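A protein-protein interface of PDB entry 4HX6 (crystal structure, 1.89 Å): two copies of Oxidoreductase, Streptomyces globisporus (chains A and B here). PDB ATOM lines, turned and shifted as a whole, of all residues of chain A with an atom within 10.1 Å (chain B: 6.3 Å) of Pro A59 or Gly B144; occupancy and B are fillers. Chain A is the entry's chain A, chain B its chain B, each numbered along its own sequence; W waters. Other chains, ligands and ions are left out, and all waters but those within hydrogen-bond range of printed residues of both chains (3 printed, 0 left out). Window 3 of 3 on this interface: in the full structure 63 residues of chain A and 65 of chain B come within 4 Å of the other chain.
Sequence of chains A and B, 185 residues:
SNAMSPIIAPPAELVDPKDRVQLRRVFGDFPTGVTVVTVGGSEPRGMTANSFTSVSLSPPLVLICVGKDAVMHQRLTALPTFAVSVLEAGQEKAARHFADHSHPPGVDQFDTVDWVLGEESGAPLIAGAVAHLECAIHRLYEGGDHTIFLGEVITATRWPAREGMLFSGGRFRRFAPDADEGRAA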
ATOM      1  N   SER A  54      10.426  22.354 -23.054  1.00  0.00           N
ATOM      2  CA  SER A  54      10.679  23.792 -22.874  1.00  0.00           C
ATOM      3  C   SER A  54      12.014  24.151 -23.545  1.00  0.00           C
ATOM      4  O   SER A  54      12.996  23.411 -23.435  1.00  0.00           O
ATOM      5  CB  SER A  54      10.681  24.190 -21.403  1.00  0.00           C
ATOM      6  OG  SER A  54      11.665  23.459 -20.700  1.00  0.00           O
ATOM      7  N   VAL A  55      12.047  25.276 -24.251  1.00  0.00           N
ATOM      8  CA  VAL A  55      13.218  25.612 -25.047  1.00  0.00           C
ATOM      9  C   VAL A  55      14.009  26.807 -24.506  1.00  0.00           C
ATOM     10  O   VAL A  55      15.236  26.741 -24.383  1.00  0.00           O
ATOM     11  CB  VAL A  55      12.833  25.882 -26.510  1.00  0.00           C
ATOM     12  CG1 VAL A  55      14.068  26.256 -27.312  1.00  0.00           C
ATOM     13  CG2 VAL A  55      12.112  24.635 -27.106  1.00  0.00           C
ATOM     14  N   SER A  56      13.314  27.900 -24.207  1.00  0.00           N
ATOM     15  CA  SER A  56      13.993  29.167 -23.904  1.00  0.00           C
ATOM     16  C   SER A  56      13.189  29.941 -22.870  1.00  0.00           C
ATOM     17  O   SER A  56      11.964  29.850 -22.859  1.00  0.00           O
ATOM     18  CB  SER A  56      14.134  29.988 -25.204  1.00  0.00           C
ATOM     19  OG  SER A  56      14.730  31.278 -24.997  1.00  0.00           O
ATOM     20  N   LEU A  57      13.876  30.684 -21.998  1.00  0.00           N
ATOM     21  CA  LEU A  57      13.206  31.576 -21.050  1.00  0.00           C
ATOM     22  C   LEU A  57      12.987  32.962 -21.650  1.00  0.00           C
ATOM     23  O   LEU A  57      11.969  33.607 -21.399  1.00  0.00           O
ATOM     24  CB  LEU A  57      14.006  31.697 -19.750  1.00  0.00           C
ATOM     25  CG  LEU A  57      14.017  30.443 -18.880  1.00  0.00           C
ATOM     26  CD1 LEU A  57      14.917  30.620 -17.669  1.00  0.00           C
ATOM     27  CD2 LEU A  57      12.596  30.092 -18.444  1.00  0.00           C
ATOM     28  N   SER A  58      13.949  33.422 -22.437  1.00  0.00           N
ATOM     29  CA  SER A  58      13.859  34.746 -23.027  1.00  0.00           C
ATOM     30  C   SER A  58      14.384  34.727 -24.452  1.00  0.00           C
ATOM     31  O   SER A  58      15.595  34.699 -24.662  1.00  0.00           O
ATOM     32  CB  SER A  58      14.648  35.754 -22.188  1.00  0.00           C
ATOM     33  OG  SER A  58      14.378  37.082 -22.616  1.00  0.00           O
ATOM     34  N   PRO A  59      13.468  34.759 -25.432  1.00  0.00           N
ATOM     35  CA  PRO A  59      12.025  34.842 -25.176  1.00  0.00           C
ATOM     36  C   PRO A  59      11.481  33.508 -24.677  1.00  0.00           C
ATOM     37  O   PRO A  59      12.197  32.515 -24.739  1.00  0.00           O
ATOM     38  CB  PRO A  59      11.450  35.170 -26.558  1.00  0.00           C
ATOM     39  CG  PRO A  59      12.412  34.539 -27.506  1.00  0.00           C
ATOM     40  CD  PRO A  59      13.773  34.680 -26.872  1.00  0.00           C
ATOM     41  N   PRO A  60      10.240  33.492 -24.167  1.00  0.00           N
ATOM     42  CA  PRO A  60       9.616  32.278 -23.637  1.00  0.00           C
ATOM     43  C   PRO A  60       9.177  31.362 -24.781  1.00  0.00           C
ATOM     44  O   PRO A  60       8.236  31.687 -25.513  1.00  0.00           O
ATOM     45  CB  PRO A  60       8.396  32.814 -22.878  1.00  0.00           C
ATOM     46  CG  PRO A  60       8.078  34.098 -23.540  1.00  0.00           C
ATOM     47  CD  PRO A  60       9.389  34.681 -23.978  1.00  0.00           C
ATOM     48  N   LEU A  61       9.875  30.245 -24.949  1.00  0.00           N
ATOM     49  CA  LEU A  61       9.606  29.344 -26.079  1.00  0.00           C
ATOM     50  C   LEU A  61       9.490  27.916 -25.644  1.00  0.00           C
ATOM     51  O   LEU A  61      10.249  27.456 -24.791  1.00  0.00           O
ATOM     52  CB  LEU A  61      10.756  29.403 -27.088  1.00  0.00           C
ATOM     53  CG  LEU A  61      11.072  30.720 -27.779  1.00  0.00           C
ATOM     54  CD1 LEU A  61      12.389  30.566 -28.532  1.00  0.00           C
ATOM     55  CD2 LEU A  61       9.933  31.119 -28.704  1.00  0.00           C
ATOM     56  N   VAL A  62       8.577  27.188 -26.275  1.00  0.00           N
ATOM     57  CA  VAL A  62       8.508  25.743 -26.095  1.00  0.00           C
ATOM     58  C   VAL A  62       8.471  25.101 -27.480  1.00  0.00           C
ATOM     59  O   VAL A  62       8.270  25.797 -28.494  1.00  0.00           O
ATOM     60  CB  VAL A  62       7.237  25.344 -25.331  1.00  0.00           C
ATOM     61  CG1 VAL A  62       7.263  25.952 -23.900  1.00  0.00           C
ATOM     62  CG2 VAL A  62       6.000  25.784 -26.122  1.00  0.00           C
ATOM     63  N   LEU A  63       8.676  23.791 -27.542  1.00  0.00           N
ATOM     64  CA  LEU A  63       8.403  23.095 -28.804  1.00  0.00           C
ATOM     65  C   LEU A  63       7.556  21.845 -28.630  1.00  0.00           C
ATOM     66  O   LEU A  63       7.503  21.236 -27.543  1.00  0.00           O
ATOM     67  CB  LEU A  63       9.691  22.797 -29.606  1.00  0.00           C
ATOM     68  CG  LEU A  63      10.723  21.810 -29.020  1.00  0.00           C
ATOM     69  CD1 LEU A  63      10.281  20.360 -29.244  1.00  0.00           C
ATOM     70  CD2 LEU A  63      12.096  22.019 -29.658  1.00  0.00           C
ATOM     71  N   ALA A 136       1.828  30.862 -29.399  1.00  0.00           N
ATOM     72  CA  ALA A 136       1.736  31.262 -30.793  1.00  0.00           C
ATOM     73  C   ALA A 136       2.888  30.598 -31.522  1.00  0.00           C
ATOM     74  O   ALA A 136       4.032  30.637 -31.056  1.00  0.00           O
ATOM     75  CB  ALA A 136       1.841  32.780 -30.929  1.00  0.00           C
ATOM     76  N   HIS A 138       5.828  30.258 -33.724  1.00  0.00           N
ATOM     77  CA  HIS A 138       6.816  31.213 -34.201  1.00  0.00           C
ATOM     78  C   HIS A 138       7.607  30.641 -35.384  1.00  0.00           C
ATOM     79  O   HIS A 138       7.849  31.328 -36.376  1.00  0.00           O
ATOM     80  CB  HIS A 138       7.747  31.587 -33.042  1.00  0.00           C
ATOM     81  CG  HIS A 138       8.806  32.578 -33.412  1.00  0.00           C
ATOM     82  ND1 HIS A 138      10.146  32.362 -33.167  1.00  0.00           N
ATOM     83  CD2 HIS A 138       8.726  33.784 -34.024  1.00  0.00           C
ATOM     84  CE1 HIS A 138      10.845  33.393 -33.609  1.00  0.00           C
ATOM     85  NE2 HIS A 138      10.007  34.271 -34.130  1.00  0.00           N
ATOM     86  N   ARG A 139       8.015  29.383 -35.274  1.00  0.00           N
ATOM     87  CA  ARG A 139       8.751  28.712 -36.343  1.00  0.00           C
ATOM     88  C   ARG A 139       8.246  27.287 -36.580  1.00  0.00           C
ATOM     89  O   ARG A 139       7.773  26.621 -35.654  1.00  0.00           O
ATOM     90  CB  ARG A 139      10.250  28.654 -36.026  1.00  0.00           C
ATOM     91  CG  ARG A 139      10.971  30.017 -35.987  1.00  0.00           C
ATOM     92  CD  ARG A 139      11.188  30.578 -37.404  1.00  0.00           C
ATOM     93  NE  ARG A 139      11.849  31.890 -37.409  1.00  0.00           N
ATOM     94  CZ  ARG A 139      11.218  33.060 -37.406  1.00  0.00           C
ATOM     95  NH1 ARG A 139       9.887  33.114 -37.358  1.00  0.00           N
ATOM     96  NH2 ARG A 139      11.920  34.188 -37.439  1.00  0.00           N
ATOM     97  N   TYR A 141      10.083  23.868 -37.999  1.00  0.00           N
ATOM     98  CA  TYR A 141      11.376  23.270 -38.329  1.00  0.00           C
ATOM     99  C   TYR A 141      11.218  21.849 -38.858  1.00  0.00           C
ATOM    100  O   TYR A 141      10.365  21.102 -38.393  1.00  0.00           O
ATOM    101  CB  TYR A 141      12.249  23.237 -37.091  1.00  0.00           C
ATOM    102  CG  TYR A 141      12.672  24.607 -36.592  1.00  0.00           C
ATOM    103  CD1 TYR A 141      13.012  25.624 -37.480  1.00  0.00           C
ATOM    104  CD2 TYR A 141      12.753  24.871 -35.235  1.00  0.00           C
ATOM    105  CE1 TYR A 141      13.420  26.862 -37.018  1.00  0.00           C
ATOM    106  CE2 TYR A 141      13.165  26.107 -34.764  1.00  0.00           C
ATOM    107  CZ  TYR A 141      13.491  27.098 -35.660  1.00  0.00           C
ATOM    108  OH  TYR A 141      13.907  28.326 -35.191  1.00  0.00           O
ATOM    109  N   LEU A 150       7.859  25.415 -33.075  1.00  0.00           N
ATOM    110  CA  LEU A 150       8.413  26.220 -31.996  1.00  0.00           C
ATOM    111  C   LEU A 150       7.372  27.269 -31.576  1.00  0.00           C
ATOM    112  O   LEU A 150       6.971  28.118 -32.385  1.00  0.00           O
ATOM    113  CB  LEU A 150       9.698  26.891 -32.451  1.00  0.00           C
ATOM    114  CG  LEU A 150      10.474  27.733 -31.445  1.00  0.00           C
ATOM    115  CD1 LEU A 150      11.017  26.858 -30.320  1.00  0.00           C
ATOM    116  CD2 LEU A 150      11.602  28.479 -32.154  1.00  0.00           C
ATOM    117  N   GLY A 151       6.910  27.195 -30.331  1.00  0.00           N
ATOM    118  CA  GLY A 151       5.883  28.126 -29.868  1.00  0.00           C
ATOM    119  C   GLY A 151       6.378  29.177 -28.881  1.00  0.00           C
ATOM    120  O   GLY A 151       7.192  28.888 -28.003  1.00  0.00           O
ATOM    121  N   GLU A 152       5.870  30.398 -29.006  1.00  0.00           N
ATOM    122  CA  GLU A 152       6.156  31.444 -28.026  1.00  0.00           C
ATOM    123  C   GLU A 152       5.039  31.475 -27.006  1.00  0.00           C
ATOM    124  O   GLU A 152       3.874  31.623 -27.383  1.00  0.00           O
ATOM    125  CB  GLU A 152       6.223  32.811 -28.702  1.00  0.00           C
ATOM    126  CG  GLU A 152       6.491  33.959 -27.732  1.00  0.00           C
ATOM    127  CD  GLU A 152       6.635  35.292 -28.448  1.00  0.00           C
ATOM    128  OE1 GLU A 152       5.863  35.541 -29.402  1.00  0.00           O
ATOM    129  OE2 GLU A 152       7.525  36.085 -28.064  1.00  0.00           O
ATOM    130  N   VAL A 153       5.385  31.353 -25.727  1.00  0.00           N
ATOM    131  CA  VAL A 153       4.376  31.234 -24.673  1.00  0.00           C
ATOM    132  C   VAL A 153       3.708  32.580 -24.459  1.00  0.00           C
ATOM    133  O   VAL A 153       4.367  33.563 -24.116  1.00  0.00           O
ATOM    134  CB  VAL A 153       4.981  30.726 -23.343  1.00  0.00           C
ATOM    135  CG1 VAL A 153       3.886  30.572 -22.277  1.00  0.00           C
ATOM    136  CG2 VAL A 153       5.705  29.417 -23.576  1.00  0.00           C
ATOM    137  N   ILE A 154       2.404  32.638 -24.697  1.00  0.00           N
ATOM    138  CA  ILE A 154       1.691  33.911 -24.559  1.00  0.00           C
ATOM    139  C   ILE A 154       1.137  34.077 -23.154  1.00  0.00           C
ATOM    140  O   ILE A 154       1.194  35.155 -22.557  1.00  0.00           O
ATOM    141  CB  ILE A 154       0.536  34.024 -25.557  1.00  0.00           C
ATOM    142  CG1 ILE A 154       1.072  33.922 -26.980  1.00  0.00           C
ATOM    143  CG2 ILE A 154      -0.244  35.324 -25.331  1.00  0.00           C
ATOM    144  CD1 ILE A 154       2.321  34.755 -27.206  1.00  0.00           C
ATOM    145  N   PRO B  17       4.713  35.065 -18.600  1.00  0.00           N
ATOM    146  CA  PRO B  17       5.832  34.372 -19.252  1.00  0.00           C
ATOM    147  C   PRO B  17       7.078  35.244 -19.317  1.00  0.00           C
ATOM    148  O   PRO B  17       8.166  34.726 -19.545  1.00  0.00           O
ATOM    149  CB  PRO B  17       5.303  34.092 -20.668  1.00  0.00           C
ATOM    150  CG  PRO B  17       3.808  34.118 -20.531  1.00  0.00           C
ATOM    151  CD  PRO B  17       3.568  35.223 -19.515  1.00  0.00           C
ATOM    152  N   LEU B  23       8.059  31.602 -15.025  1.00  0.00           N
ATOM    153  CA  LEU B  23       8.106  30.735 -16.199  1.00  0.00           C
ATOM    154  C   LEU B  23       8.876  29.447 -15.893  1.00  0.00           C
ATOM    155  O   LEU B  23       8.472  28.356 -16.309  1.00  0.00           O
ATOM    156  CB  LEU B  23       8.745  31.476 -17.385  1.00  0.00           C
ATOM    157  CG  LEU B  23       8.684  30.687 -18.697  1.00  0.00           C
ATOM    158  CD1 LEU B  23       7.238  30.425 -19.083  1.00  0.00           C
ATOM    159  CD2 LEU B  23       9.411  31.437 -19.793  1.00  0.00           C
ATOM    160  N   LYS B  68      23.034  28.829 -25.429  1.00  0.00           N
ATOM    161  CA  LYS B  68      24.026  29.470 -26.280  1.00  0.00           C
ATOM    162  C   LYS B  68      25.316  29.807 -25.538  1.00  0.00           C
ATOM    163  O   LYS B  68      26.372  29.912 -26.152  1.00  0.00           O
ATOM    164  CB  LYS B  68      23.450  30.735 -26.911  1.00  0.00           C
ATOM    165  CG  LYS B  68      22.481  30.465 -28.050  1.00  0.00           C
ATOM    166  CD  LYS B  68      21.945  31.776 -28.570  1.00  0.00           C
ATOM    167  CE  LYS B  68      21.179  31.602 -29.861  1.00  0.00           C
ATOM    168  NZ  LYS B  68      20.841  32.947 -30.411  1.00  0.00           N
ATOM    169  N   GLU B 142      17.337  27.795 -34.533  1.00  0.00           N
ATOM    170  CA  GLU B 142      17.233  28.839 -33.509  1.00  0.00           C
ATOM    171  C   GLU B 142      16.176  28.477 -32.473  1.00  0.00           C
ATOM    172  O   GLU B 142      15.073  28.057 -32.828  1.00  0.00           O
ATOM    173  CB  GLU B 142      16.841  30.173 -34.152  1.00  0.00           C
ATOM    174  CG  GLU B 142      17.900  30.735 -35.100  1.00  0.00           C
ATOM    175  CD  GLU B 142      17.498  32.081 -35.698  1.00  0.00           C
ATOM    176  OE1 GLU B 142      18.410  32.877 -36.033  1.00  0.00           O
ATOM    177  OE2 GLU B 142      16.275  32.342 -35.835  1.00  0.00           O
ATOM    178  N   GLY B 143      16.512  28.668 -31.203  1.00  0.00           N
ATOM    179  CA  GLY B 143      15.592  28.425 -30.103  1.00  0.00           C
ATOM    180  C   GLY B 143      15.710  29.489 -29.014  1.00  0.00           C
ATOM    181  O   GLY B 143      15.865  29.163 -27.829  1.00  0.00           O
ATOM    182  N   GLY B 144      15.632  30.759 -29.406  1.00  0.00           N
ATOM    183  CA  GLY B 144      15.722  31.852 -28.450  1.00  0.00           C
ATOM    184  C   GLY B 144      17.093  31.891 -27.791  1.00  0.00           C
ATOM    185  O   GLY B 144      18.101  32.078 -28.471  1.00  0.00           O
ATOM    186  N   ASP B 145      17.138  31.695 -26.474  1.00  0.00           N
ATOM    187  CA  ASP B 145      18.411  31.680 -25.752  1.00  0.00           C
ATOM    188  C   ASP B 145      19.101  30.310 -25.817  1.00  0.00           C
ATOM    189  O   ASP B 145      20.187  30.121 -25.268  1.00  0.00           O
ATOM    190  CB  ASP B 145      18.253  32.171 -24.298  1.00  0.00           C
ATOM    191  CG  ASP B 145      17.259  31.340 -23.489  1.00  0.00           C
ATOM    192  OD1 ASP B 145      17.081  30.139 -23.787  1.00  0.00           O
ATOM    193  OD2 ASP B 145      16.652  31.898 -22.538  1.00  0.00           O
ATOM    194  N   HIS B 146      18.462  29.361 -26.492  1.00  0.00           N
ATOM    195  CA  HIS B 146      19.080  28.076 -26.787  1.00  0.00           C
ATOM    196  C   HIS B 146      19.225  27.855 -28.287  1.00  0.00           C
ATOM    197  O   HIS B 146      18.645  28.574 -29.104  1.00  0.00           O
ATOM    198  CB  HIS B 146      18.266  26.904 -26.191  1.00  0.00           C
ATOM    199  CG  HIS B 146      18.406  26.770 -24.704  1.00  0.00           C
ATOM    200  ND1 HIS B 146      18.186  27.824 -23.839  1.00  0.00           N
ATOM    201  CD2 HIS B 146      18.759  25.714 -23.931  1.00  0.00           C
ATOM    202  CE1 HIS B 146      18.398  27.420 -22.596  1.00  0.00           C
ATOM    203  NE2 HIS B 146      18.743  26.144 -22.625  1.00  0.00           N
ATOM    204  N   THR B 147      20.010  26.846 -28.638  1.00  0.00           N
ATOM    205  CA  THR B 147      20.005  26.322 -29.992  1.00  0.00           C
ATOM    206  C   THR B 147      19.414  24.922 -29.938  1.00  0.00           C
ATOM    207  O   THR B 147      19.650  24.168 -28.994  1.00  0.00           O
ATOM    208  CB  THR B 147      21.419  26.246 -30.585  1.00  0.00           C
ATOM    209  OG1 THR B 147      21.939  27.567 -30.724  1.00  0.00           O
ATOM    210  CG2 THR B 147      21.399  25.579 -31.955  1.00  0.00           C
HETATM  211  O   HOH W   1      14.928  34.026 -37.571  1.00  0.00           O
HETATM  212  O   HOH W   2      14.372  30.887 -36.921  1.00  0.00           O
HETATM  213  O   HOH W   3      10.769  34.863 -19.302  1.00  0.00           O
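The backbone carbonyl oxygen (O) of Val A55 sits close to a ring nitrogen (ND1) of His B146 (3.2 Å).
The side-chain hydroxyl (OG) of Ser A56 lies within hydrogen-bond range of the backbone NH (N) of Asp B145 (2.9 Å).
The backbone NH (N) of Leu A57 sits at hydrogen-bond distance from the side-chain carboxylate (OD2) of Asp B145.
The backbone NH (N) of Ser A58 lies within hydrogen-bond range of the side-chain carboxylate (OD2) of Asp B145 (3.1 Å).
OH of Tyr A141 lies within hydrogen-bond range of O of Glu B142 (2.6 Å).
The backbone NH (N) of Val A55 lies within hydrogen-bond range of the backbone carbonyl oxygen (O) of Leu A61 (2.9 Å).
The backbone carbonyl oxygen (O) of Pro A59 sits at hydrogen-bond distance from the side-chain hydroxyl (OG) of Ser A56 (2.8 Å).
O of Ser A56 lies within hydrogen-bond range of N of Leu A61 (3.0 Å).
The backbone carbonyl oxygen of Leu A150 lies within hydrogen-bond range of the backbone NH of His A138 (2.8 Å).
NZ of Lys B68 lies close to O of Gly B144 (3.5 Å).
The backbone carbonyl oxygen (O) of Asp B145 is in hydrogen-bond range of the backbone NH (N) of Lys B68 (3.1 Å).
Among the printed residues, pairs that only touch across the chains: Val A55 with Gly B143 (3.5 Å), Val A55 with Asp B145 (3.9 Å), Ser A56 with Gly B143 (3.3 Å), Ser A56 with Gly B144 (3.6 Å), Leu A57 with Leu B23 (3.7 Å), Pro A59 with Gly B144 (3.8 Å), Pro A60 with Pro B17 (3.8 Å), Pro A60 with Leu B23 (3.5 Å), Leu A61 with Gly B143 (3.5 Å), Leu A61 with Gly B144 (3.4 Å), Leu A150 with Glu B142 (3.6 Å), Val A153 with Pro B17 (3.6 Å) and Ile A154 with Pro B17 (3.5 Å).
Pro A59 touches just one residue of chain B: Gly B144.
Of chain A, only Ser A56, Pro A59 and Leu A61 come within 4 Å of Gly B144.
Of chain A, only Val A55, Ser A56 and Leu A61 come within 4 Å of Gly B143.
Of the printed residues of chain B, Val A153 touches Pro B17 (3.6 Å).
Of the printed residues of chain A, Pro B17 touches Pro A60 (3.8 Å), Val A153 (3.6 Å) and Ile A154 (3.5 Å).
Of the printed residues of chain B, Leu A150 touches Glu B142.
The nearest printed residue of chain B that does not touch Ile A154 is Leu B23 (7.7 Å).
Hydrophobic or aromatic side chains of chain A within 4 Å of the printed part of chain B: Val A55, Leu A57, Pro A59, Pro A60, Leu A61, Tyr A141, Leu A150 and Val A153.
Of the 9 printed residues of chain B, 7 touch a printed residue of chain A.
Hydrophobic or aromatic side chains of chain B that line the printed part of chain A: Pro B17, Leu B23 and His B146.
No position is printed for both chains.
Of the 18 pairs that touch across the chains among the printed residues, none has its exchanged pair printed and touching as well.
Water W3 bridges O of Pro B17 (2.6 Å) and O of Leu A57 (2.7 Å).
Water W2 lies within hydrogen-bond range of the side-chain carboxylate of Glu B142 (2.6 Å), the guanidinium group of Arg A139 (2.8 Å) and the side-chain hydroxyl of Tyr A141 (3.1 Å).
Water W1 lies within hydrogen-bond range of the side-chain carboxylate (OE2) of Glu B142 (2.8 Å) and the guanidinium group (NH2) of Arg A139 (3.0 Å).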
